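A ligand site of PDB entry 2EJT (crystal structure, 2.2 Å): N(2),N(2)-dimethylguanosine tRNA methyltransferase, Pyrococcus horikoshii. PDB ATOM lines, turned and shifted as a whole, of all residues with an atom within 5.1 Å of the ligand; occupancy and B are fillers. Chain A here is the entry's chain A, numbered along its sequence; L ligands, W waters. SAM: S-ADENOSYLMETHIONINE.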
ATOM      1  N   PHE A  27      11.465   5.785  11.662  1.00  0.00           N
ATOM      2  CA  PHE A  27      10.629   6.137  10.523  1.00  0.00           C
ATOM      3  C   PHE A  27      10.326   5.022   9.526  1.00  0.00           C
ATOM      4  O   PHE A  27      11.196   4.239   9.142  1.00  0.00           O
ATOM      5  CB  PHE A  27      11.260   7.331   9.797  1.00  0.00           C
ATOM      6  CG  PHE A  27      10.406   7.926   8.718  1.00  0.00           C
ATOM      7  CD1 PHE A  27      10.360   7.353   7.446  1.00  0.00           C
ATOM      8  CD2 PHE A  27       9.648   9.064   8.963  1.00  0.00           C
ATOM      9  CE1 PHE A  27       9.572   7.917   6.426  1.00  0.00           C
ATOM     10  CE2 PHE A  27       8.865   9.638   7.965  1.00  0.00           C
ATOM     11  CZ  PHE A  27       8.827   9.062   6.688  1.00  0.00           C
ATOM     12  N   TYR A  28       9.068   4.978   9.091  1.00  0.00           N
ATOM     13  CA  TYR A  28       8.589   4.012   8.110  1.00  0.00           C
ATOM     14  C   TYR A  28       7.401   4.613   7.368  1.00  0.00           C
ATOM     15  O   TYR A  28       6.430   5.052   7.994  1.00  0.00           O
ATOM     16  CB  TYR A  28       8.156   2.704   8.760  1.00  0.00           C
ATOM     17  CG  TYR A  28       7.546   1.747   7.765  1.00  0.00           C
ATOM     18  CD1 TYR A  28       8.345   1.117   6.804  1.00  0.00           C
ATOM     19  CD2 TYR A  28       6.167   1.530   7.721  1.00  0.00           C
ATOM     20  CE1 TYR A  28       7.783   0.308   5.828  1.00  0.00           C
ATOM     21  CE2 TYR A  28       5.592   0.717   6.745  1.00  0.00           C
ATOM     22  CZ  TYR A  28       6.407   0.108   5.798  1.00  0.00           C
ATOM     23  OH  TYR A  28       5.848  -0.668   4.810  1.00  0.00           O
ATOM     24  N   MET A  32       6.052   4.562   0.501  1.00  0.00           N
ATOM     25  CA  MET A  32       7.334   4.367  -0.171  1.00  0.00           C
ATOM     26  C   MET A  32       7.536   2.917  -0.595  1.00  0.00           C
ATOM     27  O   MET A  32       8.613   2.547  -1.057  1.00  0.00           O
ATOM     28  CB  MET A  32       8.494   4.784   0.721  1.00  0.00           C
ATOM     29  CG  MET A  32       8.648   6.285   0.908  1.00  0.00           C
ATOM     30  SD  MET A  32       8.851   7.161  -0.666  1.00  0.00           S
ATOM     31  CE  MET A  32       7.261   8.000  -0.780  1.00  0.00           C
ATOM     32  N   ARG A  36      10.331   1.378  -3.218  1.00  0.00           N
ATOM     33  CA  ARG A  36      11.144   0.196  -2.908  1.00  0.00           C
ATOM     34  C   ARG A  36      10.897  -0.930  -3.909  1.00  0.00           C
ATOM     35  O   ARG A  36      11.819  -1.682  -4.228  1.00  0.00           O
ATOM     36  CB  ARG A  36      10.889  -0.262  -1.469  1.00  0.00           C
ATOM     37  CG  ARG A  36      11.429   0.713  -0.418  1.00  0.00           C
ATOM     38  CD  ARG A  36      11.284   0.171   1.003  1.00  0.00           C
ATOM     39  NE  ARG A  36       9.931   0.312   1.554  1.00  0.00           N
ATOM     40  CZ  ARG A  36       9.459   1.411   2.121  1.00  0.00           C
ATOM     41  NH1 ARG A  36       8.221   1.442   2.600  1.00  0.00           N
ATOM     42  NH2 ARG A  36      10.228   2.495   2.222  1.00  0.00           N
ATOM     43  N   ASP A  53      22.317   0.185   1.750  1.00  0.00           N
ATOM     44  CA  ASP A  53      21.092   0.901   2.062  1.00  0.00           C
ATOM     45  C   ASP A  53      21.603   1.899   3.131  1.00  0.00           C
ATOM     46  O   ASP A  53      21.519   1.648   4.331  1.00  0.00           O
ATOM     47  CB  ASP A  53      20.070  -0.093   2.624  1.00  0.00           C
ATOM     48  CG  ASP A  53      18.812   0.582   3.149  1.00  0.00           C
ATOM     49  OD1 ASP A  53      18.595   1.779   2.887  1.00  0.00           O
ATOM     50  OD2 ASP A  53      18.022  -0.127   3.828  1.00  0.00           O
ATOM     51  N   ALA A  54      22.165   3.007   2.644  1.00  0.00           N
ATOM     52  CA  ALA A  54      22.782   4.069   3.466  1.00  0.00           C
ATOM     53  C   ALA A  54      22.007   4.604   4.680  1.00  0.00           C
ATOM     54  O   ALA A  54      22.621   4.872   5.720  1.00  0.00           O
ATOM     55  CB  ALA A  54      23.189   5.231   2.567  1.00  0.00           C
ATOM     56  N   LEU A  55      20.710   4.812   4.531  1.00  0.00           N
ATOM     57  CA  LEU A  55      19.848   5.296   5.620  1.00  0.00           C
ATOM     58  C   LEU A  55      18.624   4.384   5.629  1.00  0.00           C
ATOM     59  O   LEU A  55      17.622   4.696   4.992  1.00  0.00           O
ATOM     60  CB  LEU A  55      19.447   6.751   5.365  1.00  0.00           C
ATOM     61  CG  LEU A  55      20.588   7.728   5.066  1.00  0.00           C
ATOM     62  CD1 LEU A  55      20.754   7.864   3.577  1.00  0.00           C
ATOM     63  CD2 LEU A  55      20.298   9.090   5.665  1.00  0.00           C
ATOM     64  N   SER A  56      18.697   3.277   6.361  1.00  0.00           N
ATOM     65  CA  SER A  56      17.622   2.297   6.367  1.00  0.00           C
ATOM     66  C   SER A  56      16.474   2.375   7.374  1.00  0.00           C
ATOM     67  O   SER A  56      15.461   1.692   7.193  1.00  0.00           O
ATOM     68  CB  SER A  56      18.215   0.879   6.404  1.00  0.00           C
ATOM     69  OG  SER A  56      19.301   0.804   7.297  1.00  0.00           O
ATOM     70  N   ALA A  57      16.621   3.184   8.418  1.00  0.00           N
ATOM     71  CA  ALA A  57      15.574   3.318   9.438  1.00  0.00           C
ATOM     72  C   ALA A  57      15.166   1.969  10.013  1.00  0.00           C
ATOM     73  O   ALA A  57      15.821   1.445  10.907  1.00  0.00           O
ATOM     74  CB  ALA A  57      14.351   4.026   8.834  1.00  0.00           C
ATOM     75  N   THR A  58      14.067   1.397   9.517  1.00  0.00           N
ATOM     76  CA  THR A  58      13.614   0.101  10.017  1.00  0.00           C
ATOM     77  C   THR A  58      14.402  -1.037   9.384  1.00  0.00           C
ATOM     78  O   THR A  58      14.422  -2.160   9.896  1.00  0.00           O
ATOM     79  CB  THR A  58      12.108  -0.143   9.702  1.00  0.00           C
ATOM     80  OG1 THR A  58      11.929  -0.188   8.286  1.00  0.00           O
ATOM     81  CG2 THR A  58      11.252   0.969  10.281  1.00  0.00           C
ATOM     82  N   ILE A  60      13.823  -1.975   6.227  1.00  0.00           N
ATOM     83  CA  ILE A  60      12.971  -2.555   5.187  1.00  0.00           C
ATOM     84  C   ILE A  60      13.567  -2.613   3.785  1.00  0.00           C
ATOM     85  O   ILE A  60      13.417  -3.621   3.079  1.00  0.00           O
ATOM     86  CB  ILE A  60      11.600  -1.827   5.102  1.00  0.00           C
ATOM     87  CG1 ILE A  60      10.705  -2.481   4.052  1.00  0.00           C
ATOM     88  CG2 ILE A  60      11.799  -0.350   4.747  1.00  0.00           C
ATOM     89  CD1 ILE A  60      10.417  -3.929   4.313  1.00  0.00           C
ATOM     90  N   ARG A  61      14.246  -1.552   3.367  1.00  0.00           N
ATOM     91  CA  ARG A  61      14.838  -1.524   2.030  1.00  0.00           C
ATOM     92  C   ARG A  61      15.900  -2.615   1.884  1.00  0.00           C
ATOM     93  O   ARG A  61      15.824  -3.456   0.982  1.00  0.00           O
ATOM     94  CB  ARG A  61      15.431  -0.143   1.738  1.00  0.00           C
ATOM     95  CG  ARG A  61      15.755   0.127   0.271  1.00  0.00           C
ATOM     96  CD  ARG A  61      16.220   1.576   0.087  1.00  0.00           C
ATOM     97  NE  ARG A  61      15.159   2.534   0.377  1.00  0.00           N
ATOM     98  CZ  ARG A  61      14.381   3.108  -0.539  1.00  0.00           C
ATOM     99  NH1 ARG A  61      13.437   3.955  -0.168  1.00  0.00           N
ATOM    100  NH2 ARG A  61      14.571   2.850  -1.834  1.00  0.00           N
ATOM    101  N   ASN A  77      22.434   0.585   7.201  1.00  0.00           N
ATOM    102  CA  ASN A  77      23.040   1.596   8.050  1.00  0.00           C
ATOM    103  C   ASN A  77      22.112   2.739   8.488  1.00  0.00           C
ATOM    104  O   ASN A  77      21.261   3.202   7.722  1.00  0.00           O
ATOM    105  CB  ASN A  77      24.257   2.206   7.335  1.00  0.00           C
ATOM    106  CG  ASN A  77      24.877   3.342   8.125  1.00  0.00           C
ATOM    107  OD1 ASN A  77      25.629   3.117   9.073  1.00  0.00           O
ATOM    108  ND2 ASN A  77      24.554   4.566   7.745  1.00  0.00           N
ATOM    109  N   ASP A  78      22.289   3.182   9.720  1.00  0.00           N
ATOM    110  CA  ASP A  78      21.534   4.296  10.264  1.00  0.00           C
ATOM    111  C   ASP A  78      22.275   4.876  11.457  1.00  0.00           C
ATOM    112  O   ASP A  78      22.877   4.157  12.235  1.00  0.00           O
ATOM    113  CB  ASP A  78      20.124   3.874  10.689  1.00  0.00           C
ATOM    114  CG  ASP A  78      19.156   5.042  10.716  1.00  0.00           C
ATOM    115  OD1 ASP A  78      18.356   5.165   9.763  1.00  0.00           O
ATOM    116  OD2 ASP A  78      19.207   5.853  11.671  1.00  0.00           O
ATOM    117  N   ILE A  79      22.205   6.191  11.584  1.00  0.00           N
ATOM    118  CA  ILE A  79      22.883   6.873  12.668  1.00  0.00           C
ATOM    119  C   ILE A  79      22.120   6.773  13.988  1.00  0.00           C
ATOM    120  O   ILE A  79      22.682   6.912  15.070  1.00  0.00           O
ATOM    121  CB  ILE A  79      23.092   8.361  12.305  1.00  0.00           C
ATOM    122  CG1 ILE A  79      24.197   8.960  13.173  1.00  0.00           C
ATOM    123  CG2 ILE A  79      21.789   9.130  12.471  1.00  0.00           C
ATOM    124  CD1 ILE A  79      24.559  10.391  12.787  1.00  0.00           C
ATOM    125  N   SER A  80      20.815   6.502  13.896  1.00  0.00           N
ATOM    126  CA  SER A  80      19.981   6.389  15.077  1.00  0.00           C
ATOM    127  C   SER A  80      20.141   5.070  15.821  1.00  0.00           C
ATOM    128  O   SER A  80      20.057   3.997  15.229  1.00  0.00           O
ATOM    129  CB  SER A  80      18.511   6.557  14.688  1.00  0.00           C
ATOM    130  OG  SER A  80      17.664   6.226  15.787  1.00  0.00           O
ATOM    131  N   ALA A  83      16.936   3.082  15.508  1.00  0.00           N
ATOM    132  CA  ALA A  83      16.816   2.476  14.178  1.00  0.00           C
ATOM    133  C   ALA A  83      17.720   1.247  14.104  1.00  0.00           C
ATOM    134  O   ALA A  83      17.309   0.205  13.603  1.00  0.00           O
ATOM    135  CB  ALA A  83      17.203   3.490  13.096  1.00  0.00           C
ATOM    136  N   ASP A 119      25.925   4.097  12.385  1.00  0.00           N
ATOM    137  CA  ASP A 119      26.916   5.124  12.116  1.00  0.00           C
ATOM    138  C   ASP A 119      26.426   6.185  11.131  1.00  0.00           C
ATOM    139  O   ASP A 119      25.339   6.072  10.558  1.00  0.00           O
ATOM    140  CB  ASP A 119      28.177   4.476  11.544  1.00  0.00           C
ATOM    141  CG  ASP A 119      29.413   5.353  11.665  1.00  0.00           C
ATOM    142  OD1 ASP A 119      30.456   4.977  11.098  1.00  0.00           O
ATOM    143  OD2 ASP A 119      29.350   6.409  12.325  1.00  0.00           O
ATOM    144  N   ASP A 120      27.242   7.213  10.956  1.00  0.00           N
ATOM    145  CA  ASP A 120      26.952   8.288  10.022  1.00  0.00           C
ATOM    146  C   ASP A 120      27.179   7.643   8.655  1.00  0.00           C
ATOM    147  O   ASP A 120      28.219   7.004   8.439  1.00  0.00           O
ATOM    148  CB  ASP A 120      27.942   9.438  10.201  1.00  0.00           C
ATOM    149  CG  ASP A 120      27.617  10.650   9.335  1.00  0.00           C
ATOM    150  OD1 ASP A 120      26.814  10.519   8.390  1.00  0.00           O
ATOM    151  OD2 ASP A 120      28.158  11.730   9.600  1.00  0.00           O
ATOM    152  N   ALA A 121      26.229   7.797   7.743  1.00  0.00           N
ATOM    153  CA  ALA A 121      26.355   7.236   6.405  1.00  0.00           C
ATOM    154  C   ALA A 121      27.652   7.708   5.746  1.00  0.00           C
ATOM    155  O   ALA A 121      28.312   6.938   5.059  1.00  0.00           O
ATOM    156  CB  ALA A 121      25.149   7.628   5.551  1.00  0.00           C
ATOM    157  N   ASN A 122      27.998   8.979   5.962  1.00  0.00           N
ATOM    158  CA  ASN A 122      29.220   9.532   5.375  1.00  0.00           C
ATOM    159  C   ASN A 122      30.473   8.857   5.914  1.00  0.00           C
ATOM    160  O   ASN A 122      31.456   8.700   5.204  1.00  0.00           O
ATOM    161  CB  ASN A 122      29.318  11.053   5.599  1.00  0.00           C
ATOM    162  CG  ASN A 122      28.571  11.844   4.547  1.00  0.00           C
ATOM    163  OD1 ASN A 122      28.705  11.574   3.359  1.00  0.00           O
ATOM    164  ND2 ASN A 122      27.787  12.825   4.981  1.00  0.00           N
ATOM    165  N   ASP A 138      18.372   7.133   0.315  1.00  0.00           N
ATOM    166  CA  ASP A 138      16.977   7.520   0.531  1.00  0.00           C
ATOM    167  C   ASP A 138      16.836   8.317   1.822  1.00  0.00           C
ATOM    168  O   ASP A 138      16.394   7.787   2.845  1.00  0.00           O
ATOM    169  CB  ASP A 138      16.102   6.269   0.596  1.00  0.00           C
ATOM    170  CG  ASP A 138      14.631   6.606   0.780  1.00  0.00           C
ATOM    171  OD1 ASP A 138      14.011   6.081   1.718  1.00  0.00           O
ATOM    172  OD2 ASP A 138      14.107   7.399  -0.030  1.00  0.00           O
ATOM    173  N   PRO A 139      17.189   9.613   1.792  1.00  0.00           N
ATOM    174  CA  PRO A 139      17.097  10.448   2.988  1.00  0.00           C
ATOM    175  C   PRO A 139      15.734  11.129   3.165  1.00  0.00           C
ATOM    176  O   PRO A 139      14.858  11.051   2.309  1.00  0.00           O
ATOM    177  CB  PRO A 139      18.197  11.468   2.757  1.00  0.00           C
ATOM    178  CG  PRO A 139      18.040  11.746   1.291  1.00  0.00           C
ATOM    179  CD  PRO A 139      17.848  10.349   0.695  1.00  0.00           C
ATOM    180  N   PHE A 140      15.589  11.782   4.313  1.00  0.00           N
ATOM    181  CA  PHE A 140      14.375  12.525   4.591  1.00  0.00           C
ATOM    182  C   PHE A 140      14.700  13.943   4.136  1.00  0.00           C
ATOM    183  O   PHE A 140      15.260  14.740   4.892  1.00  0.00           O
ATOM    184  CB  PHE A 140      14.054  12.497   6.094  1.00  0.00           C
ATOM    185  CG  PHE A 140      12.717  13.085   6.430  1.00  0.00           C
ATOM    186  CD1 PHE A 140      12.595  14.419   6.788  1.00  0.00           C
ATOM    187  CD2 PHE A 140      11.572  12.300   6.344  1.00  0.00           C
ATOM    188  CE1 PHE A 140      11.341  14.971   7.061  1.00  0.00           C
ATOM    189  CE2 PHE A 140      10.312  12.845   6.613  1.00  0.00           C
ATOM    190  CZ  PHE A 140      10.195  14.186   6.976  1.00  0.00           C
ATOM    191  N   PHE A 146      25.250  13.625   1.346  1.00  0.00           N
ATOM    192  CA  PHE A 146      25.795  12.274   1.223  1.00  0.00           C
ATOM    193  C   PHE A 146      26.304  11.940  -0.174  1.00  0.00           C
ATOM    194  O   PHE A 146      27.038  10.974  -0.352  1.00  0.00           O
ATOM    195  CB  PHE A 146      24.721  11.242   1.574  1.00  0.00           C
ATOM    196  CG  PHE A 146      24.092  11.458   2.921  1.00  0.00           C
ATOM    197  CD1 PHE A 146      24.837  11.269   4.086  1.00  0.00           C
ATOM    198  CD2 PHE A 146      22.772  11.868   3.033  1.00  0.00           C
ATOM    199  CE1 PHE A 146      24.270  11.484   5.341  1.00  0.00           C
ATOM    200  CE2 PHE A 146      22.199  12.096   4.273  1.00  0.00           C
ATOM    201  CZ  PHE A 146      22.944  11.907   5.438  1.00  0.00           C
HETATM  202  N   SAM L   1      15.465   3.960   3.614  1.00  0.00           N
HETATM  203  CA  SAM L   1      14.148   3.999   3.933  1.00  0.00           C
HETATM  204  C   SAM L   1      12.994   3.227   3.640  1.00  0.00           C
HETATM  205  O   SAM L   1      12.272   3.117   4.726  1.00  0.00           O
HETATM  206  OXT SAM L   1      12.779   2.776   2.485  1.00  0.00           O
HETATM  207  CB  SAM L   1      14.174   5.277   4.845  1.00  0.00           C
HETATM  208  CG  SAM L   1      14.813   6.448   5.534  1.00  0.00           C
HETATM  209  SD  SAM L   1      14.392   7.767   6.576  1.00  0.00           S
HETATM  210  CE  SAM L   1      13.107   8.714   5.778  1.00  0.00           C
HETATM  211  C5' SAM L   1      15.900   8.533   6.749  1.00  0.00           C
HETATM  212  C4' SAM L   1      16.491   8.366   8.214  1.00  0.00           C
HETATM  213  O4' SAM L   1      17.846   8.739   7.975  1.00  0.00           O
HETATM  214  C3' SAM L   1      16.399   7.843   9.632  1.00  0.00           C
HETATM  215  O3' SAM L   1      16.173   6.463  10.086  1.00  0.00           O
HETATM  216  C2' SAM L   1      17.646   8.408  10.319  1.00  0.00           C
HETATM  217  O2' SAM L   1      17.950   8.437  11.592  1.00  0.00           O
HETATM  218  C1' SAM L   1      18.514   8.968   9.211  1.00  0.00           C
HETATM  219  N9  SAM L   1      19.909   9.739   9.136  1.00  0.00           N
HETATM  220  C8  SAM L   1      20.047  11.052   9.242  1.00  0.00           C
HETATM  221  N7  SAM L   1      21.300  11.376   9.135  1.00  0.00           N
HETATM  222  C5  SAM L   1      22.015  10.287   8.950  1.00  0.00           C
HETATM  223  C6  SAM L   1      23.384  10.032   8.779  1.00  0.00           C
HETATM  224  N6  SAM L   1      24.255  11.038   8.773  1.00  0.00           N
HETATM  225  N1  SAM L   1      23.828   8.730   8.611  1.00  0.00           N
HETATM  226  C2  SAM L   1      22.946   7.689   8.618  1.00  0.00           C
HETATM  227  N3  SAM L   1      21.612   7.907   8.784  1.00  0.00           N
HETATM  228  C4  SAM L   1      21.119   9.199   8.960  1.00  0.00           C
HETATM  229  O   HOH W   1      15.410   0.740   4.672  1.00  0.00           O
HETATM  230  O   HOH W   2       9.897   4.333   4.611  1.00  0.00           O
HETATM  231  O   HOH W   3      14.300   6.643  11.938  1.00  0.00           O
HETATM  232  O   HOH W   4      15.398   8.223  13.739  1.00  0.00           O
HETATM  233  O   HOH W   5      18.228  10.501  13.417  1.00  0.00           O
HETATM  234  O   HOH W   6      11.864   2.235   7.346  1.00  0.00           O
HETATM  235  O   HOH W   7      24.478  14.309   8.959  1.00  0.00           O
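N of Ala 57 is in hydrogen-bond range of OD1 of Asp 78 (3.0 Å). O of Asp 78 sits at hydrogen-bond distance from N of Asp 119, 3.1 Å away. OD2 of Asp 78 lies within hydrogen-bond range of N of Ser 80, 2.8 Å away. OD1 of Asp 120 lies within hydrogen-bond range of N of Asn 122, at 3.1 Å. The backbone NH of Ile 79 sits at hydrogen-bond distance from the backbone carbonyl oxygen of Asp 119, at 3.3 Å. O of Asn 77 lies within hydrogen-bond range of N of Ser 56, at 2.9 Å. ND2 of Asn 77 sits at hydrogen-bond distance from O of Ala 54, 2.8 Å away. The side-chain hydroxyl (OG) of Ser 80 lies within hydrogen-bond range of the backbone NH (N) of Ala 83 (3.2 Å).
Water W3 bridges O3' of the ligand (2.6 Å) and N of Phe 27 (3.0 Å). Water W2 lies within hydrogen-bond range of O of the ligand and NH2 of Arg 36. Water W6 lies within hydrogen-bond range of the side-chain hydroxyl (OG1) of Thr 58 (2.6 Å), the backbone carbonyl oxygen (O) of Phe 27 (2.8 Å) and an oxygen (O) of the ligand (2.8 Å). Water W1 lies within hydrogen-bond range of O of Ser 56 (2.7 Å), OD2 of Asp 53 (2.9 Å), N of Arg 61 (2.9 Å) and N of the ligand (3.4 Å).
O3' of the ligand sits at hydrogen-bond distance from OD1 of Asp 78 (2.6 Å). NH2 of Arg 36 is in salt-bridge range of OXT of the ligand, 2.6 Å away. OD1 of Asp 120 lies within hydrogen-bond range of N6 of the ligand. A nitrogen (N) of the ligand lies within hydrogen-bond range of the backbone carbonyl oxygen (O) of Leu 55 (2.7 Å). N of Ala 121 sits at hydrogen-bond distance from N1 of the ligand, 2.7 Å away. NH1 of Arg 61 is in salt-bridge range of OXT of the ligand (3.0 Å). OD1 of Asp 138 is in salt-bridge range of N of the ligand (3.2 Å). The backbone NH (N) of Ile 79 sits at hydrogen-bond distance from a nitrogen (N3) of the ligand (3.3 Å). OD1 of Asp 53 is in salt-bridge range of N of the ligand (3.9 Å).
Phe 27 touches the ligand. Ser 56 touches the ligand (CA to N, 3.9 Å). Ala 57 touches the ligand (CA to O3', 3.3 Å). Ile 60 touches the ligand (CG2 to O, 3.5 Å). Asn 77 touches the ligand. Ser 80 touches the ligand (CB to O2', 3.7 Å). Asp 119 touches the ligand (O to C2, 3.5 Å). Phe 140 touches the ligand. CE1 of Phe 146 touches N6 of the ligand, 3.5 Å away. 18 residues have an atom within 4 Å of the ligand: Phe 27, Arg 36, Asp 53, Leu 55, Ser 56, Ala 57, Ile 60, Arg 61, Asn 77, Asp 78, Ile 79, Ser 80, Asp 119, Asp 120, Ala 121, Asp 138, Phe 140 and Phe 146. The nearest printed residue that does not touch the ligand is Ala 54 (4.1 Å).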
